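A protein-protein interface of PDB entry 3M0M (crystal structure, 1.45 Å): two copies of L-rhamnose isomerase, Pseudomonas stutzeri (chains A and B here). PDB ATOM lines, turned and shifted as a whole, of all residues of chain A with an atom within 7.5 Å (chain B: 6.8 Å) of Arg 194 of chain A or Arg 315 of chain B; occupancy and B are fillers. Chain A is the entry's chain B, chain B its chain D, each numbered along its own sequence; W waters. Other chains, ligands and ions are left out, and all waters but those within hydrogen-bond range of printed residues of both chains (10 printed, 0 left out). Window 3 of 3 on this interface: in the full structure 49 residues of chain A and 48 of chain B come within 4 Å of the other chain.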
ATOM      1  N   SER A 147      -2.254 -11.320  -0.358  1.00  0.00           N
ATOM      2  CA  SER A 147      -2.841 -11.547   0.962  1.00  0.00           C
ATOM      3  C   SER A 147      -4.163 -10.800   1.154  1.00  0.00           C
ATOM      4  O   SER A 147      -4.675 -10.708   2.268  1.00  0.00           O
ATOM      5  CB  SER A 147      -1.854 -11.146   2.068  1.00  0.00           C
ATOM      6  OG  SER A 147      -1.646  -9.743   2.104  1.00  0.00           O
ATOM      7  N   HIS A 148      -4.713 -10.271   0.065  1.00  0.00           N
ATOM      8  CA  HIS A 148      -5.979  -9.534   0.116  1.00  0.00           C
ATOM      9  C   HIS A 148      -7.079 -10.443   0.670  1.00  0.00           C
ATOM     10  O   HIS A 148      -7.041 -11.654   0.479  1.00  0.00           O
ATOM     11  CB  HIS A 148      -6.348  -9.055  -1.295  1.00  0.00           C
ATOM     12  CG  HIS A 148      -7.380  -7.967  -1.328  1.00  0.00           C
ATOM     13  ND1 HIS A 148      -8.707  -8.183  -1.020  1.00  0.00           N
ATOM     14  CD2 HIS A 148      -7.277  -6.654  -1.644  1.00  0.00           C
ATOM     15  CE1 HIS A 148      -9.376  -7.050  -1.147  1.00  0.00           C
ATOM     16  NE2 HIS A 148      -8.531  -6.107  -1.524  1.00  0.00           N
ATOM     17  N   THR A 149      -8.059  -9.865   1.359  1.00  0.00           N
ATOM     18  CA  THR A 149      -9.146 -10.662   1.922  1.00  0.00           C
ATOM     19  C   THR A 149     -10.068 -11.241   0.850  1.00  0.00           C
ATOM     20  O   THR A 149     -10.725 -12.254   1.073  1.00  0.00           O
ATOM     21  CB  THR A 149     -10.007  -9.833   2.899  1.00  0.00           C
ATOM     22  OG1 THR A 149     -10.521  -8.678   2.227  1.00  0.00           O
ATOM     23  CG2 THR A 149      -9.182  -9.394   4.099  1.00  0.00           C
ATOM     24  N   SER A 190      -5.795  -5.243   9.865  1.00  0.00           N
ATOM     25  CA  SER A 190      -5.529  -6.603   9.397  1.00  0.00           C
ATOM     26  C   SER A 190      -5.347  -7.548  10.569  1.00  0.00           C
ATOM     27  O   SER A 190      -4.938  -7.139  11.659  1.00  0.00           O
ATOM     28  CB  SER A 190      -4.224  -6.676   8.584  1.00  0.00           C
ATOM     29  OG  SER A 190      -4.170  -5.745   7.525  1.00  0.00           O
ATOM     30  N   ASN A 191      -5.663  -8.815  10.344  1.00  0.00           N
ATOM     31  CA  ASN A 191      -5.418  -9.825  11.356  1.00  0.00           C
ATOM     32  C   ASN A 191      -4.073 -10.376  10.867  1.00  0.00           C
ATOM     33  O   ASN A 191      -3.999 -11.001   9.807  1.00  0.00           O
ATOM     34  CB  ASN A 191      -6.486 -10.917  11.334  1.00  0.00           C
ATOM     35  CG  ASN A 191      -6.219 -11.999  12.356  1.00  0.00           C
ATOM     36  OD1 ASN A 191      -5.272 -12.776  12.221  1.00  0.00           O
ATOM     37  ND2 ASN A 191      -7.042 -12.046  13.402  1.00  0.00           N
ATOM     38  N   PHE A 192      -3.009 -10.114  11.625  1.00  0.00           N
ATOM     39  CA  PHE A 192      -1.666 -10.540  11.234  1.00  0.00           C
ATOM     40  C   PHE A 192      -1.560 -11.978  10.762  1.00  0.00           C
ATOM     41  O   PHE A 192      -0.974 -12.262   9.717  1.00  0.00           O
ATOM     42  CB  PHE A 192      -0.668 -10.364  12.385  1.00  0.00           C
ATOM     43  CG  PHE A 192      -0.527  -8.954  12.885  1.00  0.00           C
ATOM     44  CD1 PHE A 192      -0.675  -7.862  12.031  1.00  0.00           C
ATOM     45  CD2 PHE A 192      -0.190  -8.722  14.213  1.00  0.00           C
ATOM     46  CE1 PHE A 192      -0.487  -6.559  12.503  1.00  0.00           C
ATOM     47  CE2 PHE A 192       0.001  -7.437  14.691  1.00  0.00           C
ATOM     48  CZ  PHE A 192      -0.146  -6.348  13.835  1.00  0.00           C
ATOM     49  N   THR A 193      -2.112 -12.892  11.549  1.00  0.00           N
ATOM     50  CA  THR A 193      -2.032 -14.302  11.216  1.00  0.00           C
ATOM     51  C   THR A 193      -2.831 -14.691   9.981  1.00  0.00           C
ATOM     52  O   THR A 193      -2.303 -15.357   9.089  1.00  0.00           O
ATOM     53  CB  THR A 193      -2.457 -15.160  12.417  1.00  0.00           C
ATOM     54  OG1 THR A 193      -1.532 -14.951  13.493  1.00  0.00           O
ATOM     55  CG2 THR A 193      -2.464 -16.635  12.051  1.00  0.00           C
ATOM     56  N   ARG A 194      -4.089 -14.273   9.908  1.00  0.00           N
ATOM     57  CA  ARG A 194      -4.901 -14.618   8.748  1.00  0.00           C
ATOM     58  C   ARG A 194      -4.319 -14.053   7.454  1.00  0.00           C
ATOM     59  O   ARG A 194      -4.333 -14.725   6.427  1.00  0.00           O
ATOM     60  CB  ARG A 194      -6.344 -14.142   8.929  1.00  0.00           C
ATOM     61  CG  ARG A 194      -7.111 -14.934   9.981  1.00  0.00           C
ATOM     62  CD  ARG A 194      -8.613 -14.859   9.743  1.00  0.00           C
ATOM     63  NE  ARG A 194      -9.365 -15.643  10.719  1.00  0.00           N
ATOM     64  CZ  ARG A 194      -9.599 -15.260  11.970  1.00  0.00           C
ATOM     65  NH1 ARG A 194      -9.145 -14.094  12.405  1.00  0.00           N
ATOM     66  NH2 ARG A 194     -10.286 -16.048  12.789  1.00  0.00           N
ATOM     67  N   ALA A 195      -3.810 -12.825   7.496  1.00  0.00           N
ATOM     68  CA  ALA A 195      -3.220 -12.224   6.305  1.00  0.00           C
ATOM     69  C   ALA A 195      -2.015 -13.040   5.843  1.00  0.00           C
ATOM     70  O   ALA A 195      -1.826 -13.269   4.644  1.00  0.00           O
ATOM     71  CB  ALA A 195      -2.800 -10.786   6.593  1.00  0.00           C
ATOM     72  N   PHE A 196      -1.204 -13.490   6.795  1.00  0.00           N
ATOM     73  CA  PHE A 196      -0.026 -14.277   6.445  1.00  0.00           C
ATOM     74  C   PHE A 196      -0.443 -15.645   5.902  1.00  0.00           C
ATOM     75  O   PHE A 196       0.189 -16.174   4.986  1.00  0.00           O
ATOM     76  CB  PHE A 196       0.892 -14.416   7.664  1.00  0.00           C
ATOM     77  CG  PHE A 196       2.229 -15.045   7.359  1.00  0.00           C
ATOM     78  CD1 PHE A 196       2.932 -14.707   6.204  1.00  0.00           C
ATOM     79  CD2 PHE A 196       2.797 -15.946   8.247  1.00  0.00           C
ATOM     80  CE1 PHE A 196       4.186 -15.268   5.944  1.00  0.00           C
ATOM     81  CE2 PHE A 196       4.045 -16.507   7.996  1.00  0.00           C
ATOM     82  CZ  PHE A 196       4.741 -16.167   6.843  1.00  0.00           C
ATOM     83  N   GLU A 197      -1.515 -16.210   6.451  1.00  0.00           N
ATOM     84  CA  GLU A 197      -2.000 -17.501   5.968  1.00  0.00           C
ATOM     85  C   GLU A 197      -2.452 -17.357   4.515  1.00  0.00           C
ATOM     86  O   GLU A 197      -2.184 -18.227   3.683  1.00  0.00           O
ATOM     87  CB  GLU A 197      -3.168 -18.005   6.826  1.00  0.00           C
ATOM     88  CG  GLU A 197      -2.802 -18.330   8.269  1.00  0.00           C
ATOM     89  CD  GLU A 197      -3.995 -18.793   9.091  1.00  0.00           C
ATOM     90  OE1 GLU A 197      -5.098 -18.233   8.916  1.00  0.00           O
ATOM     91  OE2 GLU A 197      -3.828 -19.711   9.926  1.00  0.00           O
ATOM     92  N   ARG A 198      -3.128 -16.253   4.202  1.00  0.00           N
ATOM     93  CA  ARG A 198      -3.592 -16.031   2.837  1.00  0.00           C
ATOM     94  C   ARG A 198      -2.400 -15.882   1.898  1.00  0.00           C
ATOM     95  O   ARG A 198      -2.398 -16.422   0.793  1.00  0.00           O
ATOM     96  CB  ARG A 198      -4.480 -14.781   2.761  1.00  0.00           C
ATOM     97  CG  ARG A 198      -5.803 -14.918   3.505  1.00  0.00           C
ATOM     98  CD  ARG A 198      -6.733 -13.755   3.188  1.00  0.00           C
ATOM     99  NE  ARG A 198      -6.294 -12.478   3.751  1.00  0.00           N
ATOM    100  CZ  ARG A 198      -6.609 -12.048   4.970  1.00  0.00           C
ATOM    101  NH1 ARG A 198      -7.364 -12.792   5.769  1.00  0.00           N
ATOM    102  NH2 ARG A 198      -6.195 -10.856   5.382  1.00  0.00           N
ATOM    103  N   TYR A 199      -1.385 -15.149   2.346  1.00  0.00           N
ATOM    104  CA  TYR A 199      -0.178 -14.944   1.552  1.00  0.00           C
ATOM    105  C   TYR A 199       0.511 -16.277   1.251  1.00  0.00           C
ATOM    106  O   TYR A 199       0.885 -16.547   0.111  1.00  0.00           O
ATOM    107  CB  TYR A 199       0.782 -14.009   2.297  1.00  0.00           C
ATOM    108  CG  TYR A 199       2.173 -13.917   1.695  1.00  0.00           C
ATOM    109  CD1 TYR A 199       3.164 -14.838   2.032  1.00  0.00           C
ATOM    110  CD2 TYR A 199       2.495 -12.906   0.788  1.00  0.00           C
ATOM    111  CE1 TYR A 199       4.443 -14.757   1.484  1.00  0.00           C
ATOM    112  CE2 TYR A 199       3.768 -12.818   0.231  1.00  0.00           C
ATOM    113  CZ  TYR A 199       4.739 -13.743   0.583  1.00  0.00           C
ATOM    114  OH  TYR A 199       6.001 -13.647   0.037  1.00  0.00           O
ATOM    115  N   LEU A 200       0.670 -17.110   2.272  1.00  0.00           N
ATOM    116  CA  LEU A 200       1.327 -18.401   2.094  1.00  0.00           C
ATOM    117  C   LEU A 200       0.578 -19.303   1.120  1.00  0.00           C
ATOM    118  O   LEU A 200       1.196 -20.025   0.334  1.00  0.00           O
ATOM    119  CB  LEU A 200       1.481 -19.104   3.442  1.00  0.00           C
ATOM    120  CG  LEU A 200       2.497 -18.470   4.397  1.00  0.00           C
ATOM    121  CD1 LEU A 200       2.385 -19.132   5.758  1.00  0.00           C
ATOM    122  CD2 LEU A 200       3.909 -18.610   3.835  1.00  0.00           C
ATOM    123  N   ALA B 269       2.461 -12.520  17.126  1.00  0.00           N
ATOM    124  CA  ALA B 269       1.529 -13.258  16.285  1.00  0.00           C
ATOM    125  C   ALA B 269       2.225 -14.365  15.497  1.00  0.00           C
ATOM    126  O   ALA B 269       1.714 -15.483  15.407  1.00  0.00           O
ATOM    127  CB  ALA B 269       0.819 -12.305  15.328  1.00  0.00           C
ATOM    128  N   ARG B 270       3.391 -14.062  14.930  1.00  0.00           N
ATOM    129  CA  ARG B 270       4.131 -15.044  14.142  1.00  0.00           C
ATOM    130  C   ARG B 270       4.560 -16.243  14.980  1.00  0.00           C
ATOM    131  O   ARG B 270       4.407 -17.393  14.558  1.00  0.00           O
ATOM    132  CB  ARG B 270       5.362 -14.392  13.506  1.00  0.00           C
ATOM    133  CG  ARG B 270       5.042 -13.343  12.442  1.00  0.00           C
ATOM    134  CD  ARG B 270       4.659 -13.984  11.105  1.00  0.00           C
ATOM    135  NE  ARG B 270       4.442 -12.994  10.052  1.00  0.00           N
ATOM    136  CZ  ARG B 270       3.277 -12.405   9.797  1.00  0.00           C
ATOM    137  NH1 ARG B 270       2.202 -12.700  10.517  1.00  0.00           N
ATOM    138  NH2 ARG B 270       3.188 -11.517   8.815  1.00  0.00           N
ATOM    139  N   ILE B 272       3.199 -17.356  17.681  1.00  0.00           N
ATOM    140  CA  ILE B 272       2.018 -18.121  18.079  1.00  0.00           C
ATOM    141  C   ILE B 272       1.582 -19.029  16.935  1.00  0.00           C
ATOM    142  O   ILE B 272       1.278 -20.207  17.143  1.00  0.00           O
ATOM    143  CB  ILE B 272       0.839 -17.190  18.445  1.00  0.00           C
ATOM    144  CG1 ILE B 272       1.155 -16.433  19.738  1.00  0.00           C
ATOM    145  CG2 ILE B 272      -0.447 -18.008  18.597  1.00  0.00           C
ATOM    146  CD1 ILE B 272       0.127 -15.369  20.085  1.00  0.00           C
ATOM    147  N   GLN B 273       1.560 -18.481  15.725  1.00  0.00           N
ATOM    148  CA  GLN B 273       1.147 -19.248  14.557  1.00  0.00           C
ATOM    149  C   GLN B 273       2.003 -20.489  14.363  1.00  0.00           C
ATOM    150  O   GLN B 273       1.507 -21.527  13.924  1.00  0.00           O
ATOM    151  CB  GLN B 273       1.222 -18.387  13.292  1.00  0.00           C
ATOM    152  CG  GLN B 273       0.693 -19.091  12.042  1.00  0.00           C
ATOM    153  CD  GLN B 273       0.864 -18.272  10.782  1.00  0.00           C
ATOM    154  OE1 GLN B 273       1.010 -17.055  10.840  1.00  0.00           O
ATOM    155  NE2 GLN B 273       0.835 -18.937   9.633  1.00  0.00           N
ATOM    156  N   ASN B 307      -3.774  -7.875  22.611  1.00  0.00           N
ATOM    157  CA  ASN B 307      -4.812  -8.061  21.606  1.00  0.00           C
ATOM    158  C   ASN B 307      -4.484  -9.314  20.788  1.00  0.00           C
ATOM    159  O   ASN B 307      -5.376 -10.065  20.397  1.00  0.00           O
ATOM    160  CB  ASN B 307      -4.892  -6.828  20.703  1.00  0.00           C
ATOM    161  CG  ASN B 307      -5.933  -6.968  19.610  1.00  0.00           C
ATOM    162  OD1 ASN B 307      -7.098  -7.277  19.876  1.00  0.00           O
ATOM    163  ND2 ASN B 307      -5.521  -6.730  18.369  1.00  0.00           N
ATOM    164  N   GLU B 308      -3.199  -9.549  20.536  1.00  0.00           N
ATOM    165  CA  GLU B 308      -2.799 -10.732  19.785  1.00  0.00           C
ATOM    166  C   GLU B 308      -3.005 -11.997  20.616  1.00  0.00           C
ATOM    167  O   GLU B 308      -3.361 -13.045  20.085  1.00  0.00           O
ATOM    168  CB  GLU B 308      -1.330 -10.632  19.350  1.00  0.00           C
ATOM    169  CG  GLU B 308      -1.056  -9.579  18.282  1.00  0.00           C
ATOM    170  CD  GLU B 308      -1.932  -9.751  17.052  1.00  0.00           C
ATOM    171  OE1 GLU B 308      -2.061 -10.893  16.558  1.00  0.00           O
ATOM    172  OE2 GLU B 308      -2.480  -8.742  16.573  1.00  0.00           O
ATOM    173  N   LEU B 309      -2.782 -11.896  21.923  1.00  0.00           N
ATOM    174  CA  LEU B 309      -2.949 -13.047  22.797  1.00  0.00           C
ATOM    175  C   LEU B 309      -4.420 -13.435  22.877  1.00  0.00           C
ATOM    176  O   LEU B 309      -4.769 -14.616  22.802  1.00  0.00           O
ATOM    177  CB  LEU B 309      -2.401 -12.736  24.193  1.00  0.00           C
ATOM    178  CG  LEU B 309      -0.905 -12.411  24.236  1.00  0.00           C
ATOM    179  CD1 LEU B 309      -0.475 -12.130  25.668  1.00  0.00           C
ATOM    180  CD2 LEU B 309      -0.112 -13.572  23.654  1.00  0.00           C
ATOM    181  N   VAL B 310      -5.287 -12.441  23.021  1.00  0.00           N
ATOM    182  CA  VAL B 310      -6.713 -12.713  23.099  1.00  0.00           C
ATOM    183  C   VAL B 310      -7.237 -13.190  21.747  1.00  0.00           C
ATOM    184  O   VAL B 310      -8.120 -14.048  21.685  1.00  0.00           O
ATOM    185  CB  VAL B 310      -7.495 -11.469  23.564  1.00  0.00           C
ATOM    186  CG1 VAL B 310      -8.993 -11.735  23.490  1.00  0.00           C
ATOM    187  CG2 VAL B 310      -7.100 -11.119  24.993  1.00  0.00           C
ATOM    188  N   ASP B 311      -6.694 -12.648  20.661  1.00  0.00           N
ATOM    189  CA  ASP B 311      -7.133 -13.073  19.338  1.00  0.00           C
ATOM    190  C   ASP B 311      -6.811 -14.546  19.121  1.00  0.00           C
ATOM    191  O   ASP B 311      -7.575 -15.261  18.477  1.00  0.00           O
ATOM    192  CB  ASP B 311      -6.467 -12.251  18.232  1.00  0.00           C
ATOM    193  CG  ASP B 311      -6.952 -12.657  16.848  1.00  0.00           C
ATOM    194  OD1 ASP B 311      -8.179 -12.610  16.614  1.00  0.00           O
ATOM    195  OD2 ASP B 311      -6.116 -13.029  16.000  1.00  0.00           O
ATOM    196  N   ALA B 312      -5.678 -14.998  19.654  1.00  0.00           N
ATOM    197  CA  ALA B 312      -5.282 -16.394  19.507  1.00  0.00           C
ATOM    198  C   ALA B 312      -6.372 -17.281  20.092  1.00  0.00           C
ATOM    199  O   ALA B 312      -6.767 -18.277  19.489  1.00  0.00           O
ATOM    200  CB  ALA B 312      -3.963 -16.650  20.216  1.00  0.00           C
ATOM    201  N   GLU B 313      -6.865 -16.913  21.269  1.00  0.00           N
ATOM    202  CA  GLU B 313      -7.924 -17.690  21.901  1.00  0.00           C
ATOM    203  C   GLU B 313      -9.172 -17.635  21.026  1.00  0.00           C
ATOM    204  O   GLU B 313      -9.857 -18.642  20.841  1.00  0.00           O
ATOM    205  CB  GLU B 313      -8.251 -17.130  23.288  1.00  0.00           C
ATOM    206  CG  GLU B 313      -9.364 -17.890  23.995  1.00  0.00           C
ATOM    207  CD  GLU B 313      -9.754 -17.272  25.323  1.00  0.00           C
ATOM    208  OE1 GLU B 313     -10.647 -17.831  25.996  1.00  0.00           O
ATOM    209  OE2 GLU B 313      -9.176 -16.231  25.695  1.00  0.00           O
ATOM    210  N   ALA B 314      -9.452 -16.454  20.484  1.00  0.00           N
ATOM    211  CA  ALA B 314     -10.617 -16.246  19.628  1.00  0.00           C
ATOM    212  C   ALA B 314     -10.558 -17.056  18.337  1.00  0.00           C
ATOM    213  O   ALA B 314     -11.591 -17.498  17.828  1.00  0.00           O
ATOM    214  CB  ALA B 314     -10.763 -14.761  19.302  1.00  0.00           C
ATOM    215  N   ARG B 315      -9.353 -17.239  17.802  1.00  0.00           N
ATOM    216  CA  ARG B 315      -9.172 -18.001  16.571  1.00  0.00           C
ATOM    217  C   ARG B 315      -9.252 -19.498  16.843  1.00  0.00           C
ATOM    218  O   ARG B 315      -9.274 -20.303  15.911  1.00  0.00           O
ATOM    219  CB  ARG B 315      -7.815 -17.692  15.926  1.00  0.00           C
ATOM    220  CG  ARG B 315      -7.594 -16.242  15.532  1.00  0.00           C
ATOM    221  CD  ARG B 315      -6.518 -16.144  14.454  1.00  0.00           C
ATOM    222  NE  ARG B 315      -5.292 -16.860  14.811  1.00  0.00           N
ATOM    223  CZ  ARG B 315      -4.325 -16.368  15.580  1.00  0.00           C
ATOM    224  NH1 ARG B 315      -4.424 -15.144  16.083  1.00  0.00           N
ATOM    225  NH2 ARG B 315      -3.252 -17.103  15.843  1.00  0.00           N
ATOM    226  N   GLY B 316      -9.273 -19.866  18.120  1.00  0.00           N
ATOM    227  CA  GLY B 316      -9.349 -21.269  18.484  1.00  0.00           C
ATOM    228  C   GLY B 316      -8.005 -21.960  18.626  1.00  0.00           C
ATOM    229  O   GLY B 316      -7.937 -23.191  18.594  1.00  0.00           O
ATOM    230  N   VAL B 317      -6.933 -21.187  18.784  1.00  0.00           N
ATOM    231  CA  VAL B 317      -5.607 -21.776  18.942  1.00  0.00           C
ATOM    232  C   VAL B 317      -5.618 -22.629  20.205  1.00  0.00           C
ATOM    233  O   VAL B 317      -6.080 -22.188  21.259  1.00  0.00           O
ATOM    234  CB  VAL B 317      -4.513 -20.694  19.061  1.00  0.00           C
ATOM    235  CG1 VAL B 317      -3.155 -21.345  19.313  1.00  0.00           C
ATOM    236  CG2 VAL B 317      -4.466 -19.871  17.786  1.00  0.00           C
ATOM    237  N   SER B 362     -13.759  -8.608  13.108  1.00  0.00           N
ATOM    238  CA  SER B 362     -13.614  -9.545  11.996  1.00  0.00           C
ATOM    239  C   SER B 362     -14.340  -9.035  10.757  1.00  0.00           C
ATOM    240  O   SER B 362     -13.849  -9.172   9.636  1.00  0.00           O
ATOM    241  CB  SER B 362     -14.175 -10.916  12.380  1.00  0.00           C
ATOM    242  OG  SER B 362     -14.217 -11.776  11.252  1.00  0.00           O
ATOM    243  N   GLN B 365     -12.434  -6.199   9.191  1.00  0.00           N
ATOM    244  CA  GLN B 365     -11.204  -6.677   8.576  1.00  0.00           C
ATOM    245  C   GLN B 365     -11.525  -7.294   7.218  1.00  0.00           C
ATOM    246  O   GLN B 365     -10.857  -7.011   6.228  1.00  0.00           O
ATOM    247  CB  GLN B 365     -10.514  -7.706   9.479  1.00  0.00           C
ATOM    248  CG  GLN B 365     -10.074  -7.119  10.813  1.00  0.00           C
ATOM    249  CD  GLN B 365      -9.390  -8.124  11.716  1.00  0.00           C
ATOM    250  OE1 GLN B 365      -9.734  -9.305  11.723  1.00  0.00           O
ATOM    251  NE2 GLN B 365      -8.430  -7.655  12.503  1.00  0.00           N
HETATM  252  O   HOH W   1      -5.040 -10.526  15.742  1.00  0.00           O
HETATM  253  O   HOH W   2     -10.025 -11.701  10.492  1.00  0.00           O
HETATM  254  O   HOH W   3     -10.050 -13.655  15.009  1.00  0.00           O
HETATM  255  O   HOH W   4      -3.057 -12.301  14.350  1.00  0.00           O
HETATM  256  O   HOH W   5      -3.644  -8.728  14.101  1.00  0.00           O
HETATM  257  O   HOH W   6      -1.010 -15.482  16.032  1.00  0.00           O
HETATM  258  O   HOH W   7      -7.334  -9.238  14.985  1.00  0.00           O
HETATM  259  O   HOH W   8      -9.754 -10.734  13.942  1.00  0.00           O
HETATM  260  O   HOH W   9       0.603 -10.396   8.415  1.00  0.00           O
HETATM  261  O   HOH W  10       1.346 -14.780  12.293  1.00  0.00           O
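The side-chain amide nitrogen (ND2) of Asn 191 of chain A lies within hydrogen-bond range of the side-chain carboxylate (OD2) of Asp 311 of chain B (2.9 Å). O of Phe 192 of chain A is in hydrogen-bond range of NH1 of Arg 270 of chain B (3.3 Å).
The backbone NH (N) of Thr 193 of chain A is in hydrogen-bond range of the side-chain amide oxygen (OD1) of Asn 191 of chain A, at 3.2 Å. The backbone NH (N) of Arg 194 of chain A lies within hydrogen-bond range of the side-chain amide oxygen (OD1) of Asn 191 of chain A (3.0 Å). The guanidinium group (NH1) of Arg 315 of chain B is in salt-bridge range of the side-chain carboxylate (OD2) of Asp 311 of chain B (2.7 Å).
Thr 149 of chain A touches Gln 365 of chain B. NE2 of Gln 365 of chain B touches O of Ser 190 of chain A (3.6 Å). Asn 191 of chain A touches Gln 365 of chain B. Phe 192 of chain A touches Ala 269 of chain B (CB to CB, 3.8 Å). Thr 193 of chain A touches Ala 269 of chain B (OG1 to O, 3.8 Å). Gln 273 of chain B touches Thr 193 of chain A. Arg 315 of chain B touches Thr 193 of chain A. CB of Phe 196 of chain A touches NH1 of Arg 270 of chain B, at 3.6 Å. CD2 of Phe 196 of chain A touches OE1 of Gln 273 of chain B (3.3 Å). NE2 of Gln 273 of chain B touches CG of Glu 197 of chain A (3.9 Å).
Of the printed residues of chain B, Thr 149 of chain A touches Gln 365 (3.6 Å). Of the printed residues of chain B, Phe 192 of chain A touches Ala 269 (3.8 Å), Arg 270 (3.3 Å) and Glu 308 (3.3 Å). Printed residues of chain B within 4 Å of Thr 193 of chain A: Ala 269, Gln 273 and Arg 315. Printed residues of chain B within 4 Å of Arg 194 of chain A: Arg 315 (3.8 Å). Asn 307 of chain B touches none of the printed residues of chain A. Leu 309 of chain B touches none of the printed residues of chain A. No residue of chain A comes within 4 Å of Ala 314 of chain B. The nearest printed residue of chain A that does not touch Arg 270 of chain B is Thr 193 of chain A (4.4 Å).
Of the 14 printed residues of chain A, 8 touch a printed residue of chain B. Hydrophobic or aromatic side chains of chain A within 4 Å of the printed part of chain B: Phe 192 and Phe 196. Among the printed residues, 14 pairs touch across the chains. Among the printed residues, no Asp or Glu carboxylate lies within 4 Å of a Lys or Arg side-chain nitrogen of the other chain.
No position is printed for both chains. Of the 14 pairs that touch across the chains among the printed residues, none has its exchanged pair printed and touching as well.
Water W8 lies within hydrogen-bond range of OE1 of Gln 365 of chain B and ND2 of Asn 191 of chain A. Water W6 lies within hydrogen-bond range of OG1 of Thr 193 of chain A, NH2 of Arg 315 of chain B and O of Ala 269 of chain B. Water W2 lies within hydrogen-bond range of the side-chain amide oxygen of Gln 365 of chain B and the guanidinium group of Arg 194 of chain A. Water W10 lies within hydrogen-bond range of the side-chain amide oxygen (OE1) of Gln 273 of chain B (2.7 Å), the guanidinium group (NH1) of Arg 270 of chain B (2.9 Å), the side-chain hydroxyl (OG1) of Thr 193 of chain A (3.1 Å) and the backbone carbonyl oxygen (O) of Ala 269 of chain B (3.2 Å). Water W1 lies within hydrogen-bond range of OD2 of Asp 311 of chain B, OE1 of Glu 308 of chain B and ND2 of Asn 191 of chain A. Water W7 lies within hydrogen-bond range of NE2 of Gln 365 of chain B (3.1 Å) and ND2 of Asn 191 of chain A (3.2 Å).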
